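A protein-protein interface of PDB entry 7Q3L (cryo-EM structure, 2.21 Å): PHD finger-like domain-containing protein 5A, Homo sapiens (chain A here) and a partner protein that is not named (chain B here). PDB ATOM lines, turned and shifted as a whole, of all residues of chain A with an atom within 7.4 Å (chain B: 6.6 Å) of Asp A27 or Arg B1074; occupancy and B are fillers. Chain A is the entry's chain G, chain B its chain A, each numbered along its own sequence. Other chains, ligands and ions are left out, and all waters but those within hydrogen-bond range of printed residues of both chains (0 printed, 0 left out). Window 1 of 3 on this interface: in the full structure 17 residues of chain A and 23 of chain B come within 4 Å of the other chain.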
ATOM      1  N   LEU A  22       3.029  14.158  18.018  1.00  0.00           N
ATOM      2  CA  LEU A  22       3.493  13.892  16.660  1.00  0.00           C
ATOM      3  C   LEU A  22       2.611  14.608  15.640  1.00  0.00           C
ATOM      4  O   LEU A  22       1.401  14.635  15.823  1.00  0.00           O
ATOM      5  CB  LEU A  22       3.449  12.380  16.408  1.00  0.00           C
ATOM      6  CG  LEU A  22       4.595  11.560  16.992  1.00  0.00           C
ATOM      7  CD1 LEU A  22       4.449  10.100  16.594  1.00  0.00           C
ATOM      8  CD2 LEU A  22       5.946  12.104  16.551  1.00  0.00           C
ATOM      9  N   CYS A  23       3.215  15.166  14.574  1.00  0.00           N
ATOM     10  CA  CYS A  23       2.451  15.761  13.477  1.00  0.00           C
ATOM     11  C   CYS A  23       1.908  14.646  12.579  1.00  0.00           C
ATOM     12  O   CYS A  23       2.337  13.510  12.723  1.00  0.00           O
ATOM     13  CB  CYS A  23       3.324  16.709  12.659  1.00  0.00           C
ATOM     14  SG  CYS A  23       4.814  15.921  11.991  1.00  0.00           S
ATOM     15  N   GLU A  24       0.979  14.962  11.663  1.00  0.00           N
ATOM     16  CA  GLU A  24       0.320  13.946  10.845  1.00  0.00           C
ATOM     17  C   GLU A  24       1.316  13.152   9.993  1.00  0.00           C
ATOM     18  O   GLU A  24       1.180  11.933   9.870  1.00  0.00           O
ATOM     19  CB  GLU A  24      -0.791  14.554   9.985  1.00  0.00           C
ATOM     20  CG  GLU A  24      -1.720  13.518   9.362  1.00  0.00           C
ATOM     21  CD  GLU A  24      -2.403  12.601  10.364  1.00  0.00           C
ATOM     22  OE1 GLU A  24      -3.185  13.116  11.187  1.00  0.00           O
ATOM     23  OE2 GLU A  24      -2.130  11.386  10.339  1.00  0.00           O
ATOM     24  N   LYS A  25       2.299  13.841   9.393  1.00  0.00           N
ATOM     25  CA  LYS A  25       3.271  13.171   8.534  1.00  0.00           C
ATOM     26  C   LYS A  25       4.110  12.163   9.326  1.00  0.00           C
ATOM     27  O   LYS A  25       4.383  11.069   8.820  1.00  0.00           O
ATOM     28  CB  LYS A  25       4.126  14.163   7.733  1.00  0.00           C
ATOM     29  CG  LYS A  25       4.812  15.258   8.537  1.00  0.00           C
ATOM     30  CD  LYS A  25       5.630  16.209   7.697  1.00  0.00           C
ATOM     31  CE  LYS A  25       6.276  17.304   8.520  1.00  0.00           C
ATOM     32  NZ  LYS A  25       7.105  18.208   7.685  1.00  0.00           N
ATOM     33  N   CYS A  26       4.498  12.532  10.560  1.00  0.00           N
ATOM     34  CA  CYS A  26       5.302  11.668  11.419  1.00  0.00           C
ATOM     35  C   CYS A  26       4.427  10.822  12.347  1.00  0.00           C
ATOM     36  O   CYS A  26       4.956  10.099  13.193  1.00  0.00           O
ATOM     37  CB  CYS A  26       6.277  12.473  12.273  1.00  0.00           C
ATOM     38  SG  CYS A  26       7.493  13.405  11.304  1.00  0.00           S
ATOM     39  N   ASP A  27       3.095  10.898  12.182  1.00  0.00           N
ATOM     40  CA  ASP A  27       2.154  10.194  13.050  1.00  0.00           C
ATOM     41  C   ASP A  27       2.484   8.700  13.088  1.00  0.00           C
ATOM     42  O   ASP A  27       2.732   8.104  12.042  1.00  0.00           O
ATOM     43  CB  ASP A  27       0.703  10.419  12.607  1.00  0.00           C
ATOM     44  CG  ASP A  27      -0.322  10.271  13.720  1.00  0.00           C
ATOM     45  OD1 ASP A  27       0.054   9.755  14.796  1.00  0.00           O
ATOM     46  OD2 ASP A  27      -1.479  10.681  13.508  1.00  0.00           O
ATOM     47  N   GLY A  28       2.480   8.095  14.285  1.00  0.00           N
ATOM     48  CA  GLY A  28       2.756   6.675  14.434  1.00  0.00           C
ATOM     49  C   GLY A  28       4.223   6.258  14.293  1.00  0.00           C
ATOM     50  O   GLY A  28       4.510   5.079  14.437  1.00  0.00           O
ATOM     51  N   LYS A  29       5.164   7.168  14.091  1.00  0.00           N
ATOM     52  CA  LYS A  29       6.549   6.718  14.026  1.00  0.00           C
ATOM     53  C   LYS A  29       7.111   6.695  15.440  1.00  0.00           C
ATOM     54  O   LYS A  29       6.643   7.452  16.258  1.00  0.00           O
ATOM     55  CB  LYS A  29       7.380   7.778  13.314  1.00  0.00           C
ATOM     56  CG  LYS A  29       7.828   7.480  11.892  1.00  0.00           C
ATOM     57  CD  LYS A  29       8.618   8.656  11.332  1.00  0.00           C
ATOM     58  CE  LYS A  29       8.884   8.548   9.844  1.00  0.00           C
ATOM     59  NZ  LYS A  29       9.549   9.761   9.309  1.00  0.00           N
ATOM     60  N   CYS A  30       8.120   5.866  15.718  1.00  0.00           N
ATOM     61  CA  CYS A  30       8.791   5.890  17.009  1.00  0.00           C
ATOM     62  C   CYS A  30       9.874   6.935  16.899  1.00  0.00           C
ATOM     63  O   CYS A  30      10.588   6.926  15.934  1.00  0.00           O
ATOM     64  CB  CYS A  30       9.413   4.528  17.271  1.00  0.00           C
ATOM     65  SG  CYS A  30      10.541   4.354  18.678  1.00  0.00           S
ATOM     66  N   SER A  35      10.378   3.499  13.351  1.00  0.00           N
ATOM     67  CA  SER A  35       9.580   2.404  12.845  1.00  0.00           C
ATOM     68  C   SER A  35       8.126   2.732  13.111  1.00  0.00           C
ATOM     69  O   SER A  35       7.861   3.485  14.011  1.00  0.00           O
ATOM     70  CB  SER A  35       9.911   1.179  13.562  1.00  0.00           C
ATOM     71  OG  SER A  35       8.724   0.515  14.005  1.00  0.00           O
ATOM     72  N   TYR A  36       7.220   2.132  12.352  1.00  0.00           N
ATOM     73  CA  TYR A  36       5.811   2.379  12.551  1.00  0.00           C
ATOM     74  C   TYR A  36       5.192   1.142  13.183  1.00  0.00           C
ATOM     75  O   TYR A  36       3.990   1.109  13.335  1.00  0.00           O
ATOM     76  CB  TYR A  36       5.129   2.600  11.202  1.00  0.00           C
ATOM     77  CG  TYR A  36       5.373   3.914  10.520  1.00  0.00           C
ATOM     78  CD1 TYR A  36       4.618   5.025  10.847  1.00  0.00           C
ATOM     79  CD2 TYR A  36       6.293   4.023   9.491  1.00  0.00           C
ATOM     80  CE1 TYR A  36       4.809   6.230  10.205  1.00  0.00           C
ATOM     81  CE2 TYR A  36       6.499   5.226   8.842  1.00  0.00           C
ATOM     82  CZ  TYR A  36       5.744   6.330   9.194  1.00  0.00           C
ATOM     83  OH  TYR A  36       5.923   7.519   8.560  1.00  0.00           O
ATOM     84  N   CYS A  58       5.998  18.703  17.512  1.00  0.00           N
ATOM     85  CA  CYS A  58       6.181  17.298  17.141  1.00  0.00           C
ATOM     86  C   CYS A  58       7.544  16.864  17.676  1.00  0.00           C
ATOM     87  O   CYS A  58       8.505  17.625  17.524  1.00  0.00           O
ATOM     88  CB  CYS A  58       6.087  17.127  15.622  1.00  0.00           C
ATOM     89  SG  CYS A  58       6.787  15.596  14.945  1.00  0.00           S
ATOM     90  N   ILE A  60       9.654  14.519  16.733  1.00  0.00           N
ATOM     91  CA  ILE A  60      10.612  14.294  15.645  1.00  0.00           C
ATOM     92  C   ILE A  60      10.974  15.584  14.886  1.00  0.00           C
ATOM     93  O   ILE A  60      12.175  15.816  14.655  1.00  0.00           O
ATOM     94  CB  ILE A  60      10.104  13.185  14.697  1.00  0.00           C
ATOM     95  CG1 ILE A  60       9.592  11.984  15.495  1.00  0.00           C
ATOM     96  CG2 ILE A  60      11.164  12.775  13.675  1.00  0.00           C
ATOM     97  CD1 ILE A  60       9.442  10.706  14.686  1.00  0.00           C
ATOM     98  N   VAL A  66      -0.604  16.509  16.157  1.00  0.00           N
ATOM     99  CA  VAL A  66      -2.006  16.096  16.015  1.00  0.00           C
ATOM    100  C   VAL A  66      -2.303  14.839  16.849  1.00  0.00           C
ATOM    101  O   VAL A  66      -3.487  14.540  17.076  1.00  0.00           O
ATOM    102  CB  VAL A  66      -2.374  15.872  14.530  1.00  0.00           C
ATOM    103  CG1 VAL A  66      -1.857  17.002  13.654  1.00  0.00           C
ATOM    104  CG2 VAL A  66      -1.860  14.536  14.012  1.00  0.00           C
ATOM    105  N   SER A  67      -1.257  14.132  17.313  1.00  0.00           N
ATOM    106  CA  SER A  67      -1.454  12.863  18.035  1.00  0.00           C
ATOM    107  C   SER A  67      -0.348  12.668  19.076  1.00  0.00           C
ATOM    108  O   SER A  67       0.666  13.342  18.964  1.00  0.00           O
ATOM    109  CB  SER A  67      -1.493  11.690  17.087  1.00  0.00           C
ATOM    110  OG  SER A  67      -0.350  10.868  17.267  1.00  0.00           O
ATOM    111  N   ASP A  68      -0.556  11.792  20.068  1.00  0.00           N
ATOM    112  CA  ASP A  68       0.465  11.502  21.084  1.00  0.00           C
ATOM    113  C   ASP A  68       1.595  10.649  20.493  1.00  0.00           C
ATOM    114  O   ASP A  68       1.310   9.714  19.746  1.00  0.00           O
ATOM    115  CB  ASP A  68      -0.159  10.824  22.309  1.00  0.00           C
ATOM    116  CG  ASP A  68      -1.364  11.567  22.851  1.00  0.00           C
ATOM    117  OD1 ASP A  68      -1.180  12.686  23.377  1.00  0.00           O
ATOM    118  OD2 ASP A  68      -2.482  11.028  22.732  1.00  0.00           O
ATOM    119  N   ALA A  69       2.864  10.993  20.791  1.00  0.00           N
ATOM    120  CA  ALA A  69       4.010  10.201  20.347  1.00  0.00           C
ATOM    121  C   ALA A  69       4.104   8.901  21.148  1.00  0.00           C
ATOM    122  O   ALA A  69       3.802   8.908  22.348  1.00  0.00           O
ATOM    123  CB  ALA A  69       5.272  11.023  20.475  1.00  0.00           C
ATOM    124  N   ILE B1036     -10.949   2.844   1.200  1.00  0.00           N
ATOM    125  CA  ILE B1036     -10.069   1.720   1.502  1.00  0.00           C
ATOM    126  C   ILE B1036     -10.729   0.837   2.563  1.00  0.00           C
ATOM    127  O   ILE B1036     -10.793  -0.378   2.386  1.00  0.00           O
ATOM    128  CB  ILE B1036      -8.659   2.196   1.927  1.00  0.00           C
ATOM    129  CG1 ILE B1036      -7.960   2.989   0.818  1.00  0.00           C
ATOM    130  CG2 ILE B1036      -7.792   1.031   2.393  1.00  0.00           C
ATOM    131  CD1 ILE B1036      -6.871   3.926   1.304  1.00  0.00           C
ATOM    132  N   LEU B1065      -0.007   2.903  -0.776  1.00  0.00           N
ATOM    133  CA  LEU B1065      -0.723   3.515   0.340  1.00  0.00           C
ATOM    134  C   LEU B1065      -0.279   2.966   1.705  1.00  0.00           C
ATOM    135  O   LEU B1065      -0.466   3.637   2.721  1.00  0.00           O
ATOM    136  CB  LEU B1065      -2.237   3.414   0.111  1.00  0.00           C
ATOM    137  CG  LEU B1065      -2.738   3.946  -1.234  1.00  0.00           C
ATOM    138  CD1 LEU B1065      -4.225   3.670  -1.411  1.00  0.00           C
ATOM    139  CD2 LEU B1065      -2.450   5.433  -1.386  1.00  0.00           C
ATOM    140  N   LEU B1066       0.409   1.810   1.724  1.00  0.00           N
ATOM    141  CA  LEU B1066       1.062   1.252   2.909  1.00  0.00           C
ATOM    142  C   LEU B1066       2.113   2.192   3.516  1.00  0.00           C
ATOM    143  O   LEU B1066       2.458   2.031   4.688  1.00  0.00           O
ATOM    144  CB  LEU B1066       1.696  -0.099   2.554  1.00  0.00           C
ATOM    145  CG  LEU B1066       0.738  -1.237   2.190  1.00  0.00           C
ATOM    146  CD1 LEU B1066       1.509  -2.455   1.714  1.00  0.00           C
ATOM    147  CD2 LEU B1066      -0.144  -1.619   3.366  1.00  0.00           C
ATOM    148  N   LYS B1067       2.615   3.173   2.744  1.00  0.00           N
ATOM    149  CA  LYS B1067       3.589   4.154   3.210  1.00  0.00           C
ATOM    150  C   LYS B1067       3.092   5.601   3.082  1.00  0.00           C
ATOM    151  O   LYS B1067       3.888   6.540   3.177  1.00  0.00           O
ATOM    152  CB  LYS B1067       4.940   3.944   2.515  1.00  0.00           C
ATOM    153  CG  LYS B1067       5.629   2.612   2.803  1.00  0.00           C
ATOM    154  CD  LYS B1067       6.102   2.404   4.225  1.00  0.00           C
ATOM    155  CE  LYS B1067       7.309   3.243   4.581  1.00  0.00           C
ATOM    156  NZ  LYS B1067       7.812   2.910   5.932  1.00  0.00           N
ATOM    157  N   ALA B1068       1.778   5.804   2.915  1.00  0.00           N
ATOM    158  CA  ALA B1068       1.188   7.140   2.850  1.00  0.00           C
ATOM    159  C   ALA B1068       1.479   7.962   4.111  1.00  0.00           C
ATOM    160  O   ALA B1068       1.664   7.417   5.200  1.00  0.00           O
ATOM    161  CB  ALA B1068      -0.295   7.030   2.590  1.00  0.00           C
ATOM    162  N   HIS B1069       1.495   9.292   3.965  1.00  0.00           N
ATOM    163  CA  HIS B1069       1.797  10.238   5.035  1.00  0.00           C
ATOM    164  C   HIS B1069       0.841  10.083   6.228  1.00  0.00           C
ATOM    165  O   HIS B1069       1.282  10.020   7.379  1.00  0.00           O
ATOM    166  CB  HIS B1069       1.840  11.663   4.448  1.00  0.00           C
ATOM    167  CG  HIS B1069       0.478  12.195   4.154  1.00  0.00           C
ATOM    168  ND1 HIS B1069      -0.279  11.751   3.087  1.00  0.00           N
ATOM    169  CD2 HIS B1069      -0.307  13.043   4.854  1.00  0.00           C
ATOM    170  CE1 HIS B1069      -1.462  12.325   3.128  1.00  0.00           C
ATOM    171  NE2 HIS B1069      -1.507  13.116   4.205  1.00  0.00           N
ATOM    172  N   LYS B1070      -0.472   9.979   5.948  1.00  0.00           N
ATOM    173  CA  LYS B1070      -1.506   9.971   6.979  1.00  0.00           C
ATOM    174  C   LYS B1070      -1.604   8.626   7.706  1.00  0.00           C
ATOM    175  O   LYS B1070      -1.705   7.584   7.064  1.00  0.00           O
ATOM    176  CB  LYS B1070      -2.858  10.315   6.357  1.00  0.00           C
ATOM    177  CG  LYS B1070      -3.785  10.973   7.358  1.00  0.00           C
ATOM    178  CD  LYS B1070      -5.190  11.197   6.845  1.00  0.00           C
ATOM    179  CE  LYS B1070      -6.090  11.930   7.825  1.00  0.00           C
ATOM    180  NZ  LYS B1070      -5.548  13.260   8.195  1.00  0.00           N
ATOM    181  N   LYS B1071      -1.659   8.648   9.047  1.00  0.00           N
ATOM    182  CA  LYS B1071      -1.749   7.415   9.824  1.00  0.00           C
ATOM    183  C   LYS B1071      -3.015   6.608   9.509  1.00  0.00           C
ATOM    184  O   LYS B1071      -2.957   5.381   9.398  1.00  0.00           O
ATOM    185  CB  LYS B1071      -1.607   7.680  11.326  1.00  0.00           C
ATOM    186  CG  LYS B1071      -1.531   6.413  12.167  1.00  0.00           C
ATOM    187  CD  LYS B1071      -1.222   6.645  13.634  1.00  0.00           C
ATOM    188  CE  LYS B1071      -2.410   7.203  14.394  1.00  0.00           C
ATOM    189  NZ  LYS B1071      -1.996   8.023  15.555  1.00  0.00           N
ATOM    190  N   ALA B1072      -4.151   7.296   9.348  1.00  0.00           N
ATOM    191  CA  ALA B1072      -5.442   6.668   9.080  1.00  0.00           C
ATOM    192  C   ALA B1072      -5.443   5.882   7.763  1.00  0.00           C
ATOM    193  O   ALA B1072      -5.853   4.718   7.728  1.00  0.00           O
ATOM    194  CB  ALA B1072      -6.531   7.710   9.117  1.00  0.00           C
ATOM    195  N   ILE B1073      -4.921   6.500   6.693  1.00  0.00           N
ATOM    196  CA  ILE B1073      -4.795   5.882   5.375  1.00  0.00           C
ATOM    197  C   ILE B1073      -3.905   4.636   5.433  1.00  0.00           C
ATOM    198  O   ILE B1073      -4.274   3.595   4.888  1.00  0.00           O
ATOM    199  CB  ILE B1073      -4.325   6.899   4.312  1.00  0.00           C
ATOM    200  CG1 ILE B1073      -5.333   8.042   4.166  1.00  0.00           C
ATOM    201  CG2 ILE B1073      -4.035   6.220   2.972  1.00  0.00           C
ATOM    202  CD1 ILE B1073      -4.863   9.193   3.297  1.00  0.00           C
ATOM    203  N   ARG B1074      -2.754   4.706   6.119  1.00  0.00           N
ATOM    204  CA  ARG B1074      -1.896   3.538   6.282  1.00  0.00           C
ATOM    205  C   ARG B1074      -2.604   2.415   7.036  1.00  0.00           C
ATOM    206  O   ARG B1074      -2.563   1.282   6.569  1.00  0.00           O
ATOM    207  CB  ARG B1074      -0.586   3.851   7.003  1.00  0.00           C
ATOM    208  CG  ARG B1074       0.392   4.692   6.200  1.00  0.00           C
ATOM    209  CD  ARG B1074       1.790   4.669   6.804  1.00  0.00           C
ATOM    210  NE  ARG B1074       1.780   5.012   8.217  1.00  0.00           N
ATOM    211  CZ  ARG B1074       1.693   6.234   8.727  1.00  0.00           C
ATOM    212  NH1 ARG B1074       1.649   6.363  10.036  1.00  0.00           N
ATOM    213  NH2 ARG B1074       1.651   7.310   7.966  1.00  0.00           N
ATOM    214  N   ARG B1075      -3.248   2.707   8.177  1.00  0.00           N
ATOM    215  CA  ARG B1075      -3.915   1.685   8.976  1.00  0.00           C
ATOM    216  C   ARG B1075      -5.046   1.015   8.192  1.00  0.00           C
ATOM    217  O   ARG B1075      -5.182  -0.207   8.248  1.00  0.00           O
ATOM    218  CB  ARG B1075      -4.419   2.263  10.302  1.00  0.00           C
ATOM    219  CG  ARG B1075      -4.900   1.207  11.287  1.00  0.00           C
ATOM    220  CD  ARG B1075      -3.741   0.328  11.759  1.00  0.00           C
ATOM    221  NE  ARG B1075      -3.854  -1.050  11.311  1.00  0.00           N
ATOM    222  CZ  ARG B1075      -2.912  -1.994  11.404  1.00  0.00           C
ATOM    223  NH1 ARG B1075      -1.706  -1.711  11.870  1.00  0.00           N
ATOM    224  NH2 ARG B1075      -3.196  -3.231  11.043  1.00  0.00           N
ATOM    225  N   ALA B1076      -5.846   1.806   7.469  1.00  0.00           N
ATOM    226  CA  ALA B1076      -6.850   1.279   6.554  1.00  0.00           C
ATOM    227  C   ALA B1076      -6.215   0.370   5.497  1.00  0.00           C
ATOM    228  O   ALA B1076      -6.661  -0.756   5.313  1.00  0.00           O
ATOM    229  CB  ALA B1076      -7.641   2.407   5.937  1.00  0.00           C
ATOM    230  N   THR B1077      -5.129   0.810   4.848  1.00  0.00           N
ATOM    231  CA  THR B1077      -4.460  -0.007   3.841  1.00  0.00           C
ATOM    232  C   THR B1077      -3.923  -1.317   4.424  1.00  0.00           C
ATOM    233  O   THR B1077      -4.149  -2.371   3.844  1.00  0.00           O
ATOM    234  CB  THR B1077      -3.342   0.747   3.112  1.00  0.00           C
ATOM    235  OG1 THR B1077      -3.823   2.017   2.689  1.00  0.00           O
ATOM    236  CG2 THR B1077      -2.883   0.008   1.878  1.00  0.00           C
ATOM    237  N   VAL B1078      -3.271  -1.279   5.590  1.00  0.00           N
ATOM    238  CA  VAL B1078      -2.716  -2.461   6.249  1.00  0.00           C
ATOM    239  C   VAL B1078      -3.814  -3.478   6.586  1.00  0.00           C
ATOM    240  O   VAL B1078      -3.690  -4.649   6.231  1.00  0.00           O
ATOM    241  CB  VAL B1078      -1.880  -2.067   7.484  1.00  0.00           C
ATOM    242  CG1 VAL B1078      -1.472  -3.274   8.315  1.00  0.00           C
ATOM    243  CG2 VAL B1078      -0.640  -1.285   7.089  1.00  0.00           C
ATOM    244  N   ASN B1079      -4.897  -3.042   7.242  1.00  0.00           N
ATOM    245  CA  ASN B1079      -6.020  -3.902   7.606  1.00  0.00           C
ATOM    246  C   ASN B1079      -6.600  -4.607   6.373  1.00  0.00           C
ATOM    247  O   ASN B1079      -6.895  -5.803   6.392  1.00  0.00           O
ATOM    248  CB  ASN B1079      -7.135  -3.079   8.264  1.00  0.00           C
ATOM    249  CG  ASN B1079      -6.807  -2.469   9.615  1.00  0.00           C
ATOM    250  OD1 ASN B1079      -5.797  -2.791  10.241  1.00  0.00           O
ATOM    251  ND2 ASN B1079      -7.666  -1.571  10.075  1.00  0.00           N
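The side-chain carboxylate (OE1) of Glu A24 lies within salt-bridge range of the side-chain amino group (NZ) of Lys B1070 (3.8 Å).
The side-chain carboxylate (OE2) of Glu A24 lies within hydrogen-bond range of the backbone NH (N) of Lys B1071.
OD1 of Asp A27 is in salt-bridge range of NZ of Lys B1071.
The backbone carbonyl oxygen of Asp A27 lies within hydrogen-bond range of the guanidinium group of Arg B1074, 2.9 Å away.
O of His B1069 lies close to O of Glu A24, 3.1 Å away.
Cys A23 touches none of the printed residues of chain B.
Of the printed residues of chain B, Lys A25 touches His B1069.
Of chain B, only Lys B1071 and Arg B1074 come within 4 Å of Asp A27.
Lys A29 touches none of the printed residues of chain B.
Printed residues of chain A within 4 Å of His B1069: Glu A24 (3.1 Å) and Lys A25 (3.6 Å).
Of the printed residues of chain A, Lys B1071 touches Glu A24 (3.1 Å), Asp A27 (2.8 Å) and Ser A67 (3.7 Å).
Printed residues of chain A within 4 Å of Arg B1074: Asp A27 (2.9 Å) and Tyr A36 (3.2 Å).
The nearest residue of chain B that does not touch Asp A27 is His B1069 (5.2 Å).
The nearest printed residue of chain B that does not touch Lys A25 is Arg B1074 (4.7 Å).
Among the printed residues, merely in contact across the chains: Tyr A36 with Arg B1074 (3.2 Å), Lys A25 with His B1069 (3.6 Å), Ser A67 with Lys B1071 (3.7 Å) and Tyr A36 with Lys B1067 (3.9 Å).
The backbone carbonyl oxygen of Ser A67 lies within hydrogen-bond range of the backbone NH of Leu A22 (2.7 Å).
The side-chain carboxylate (OD1) of Asp A27 is in hydrogen-bond range of the side-chain hydroxyl (OG) of Ser A67.
NH2 of Arg B1074 is in hydrogen-bond range of O of Ala B1068 (2.8 Å).
The guanidinium group (NH2) of Arg B1074 sits at hydrogen-bond distance from the backbone carbonyl oxygen (O) of His B1069, 2.8 Å away.
O of Lys B1070 sits at hydrogen-bond distance from NH2 of Arg B1074 (3.5 Å).
Hydrophobic or aromatic side chains of chain A within 4 Å of the printed part of chain B: Tyr A36.
Among the printed residues, Asp or Glu carboxylates within 4 Å of a Lys or Arg side-chain nitrogen of the other chain: Glu A24 with Lys B1070 and Asp A27 with Lys B1071.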
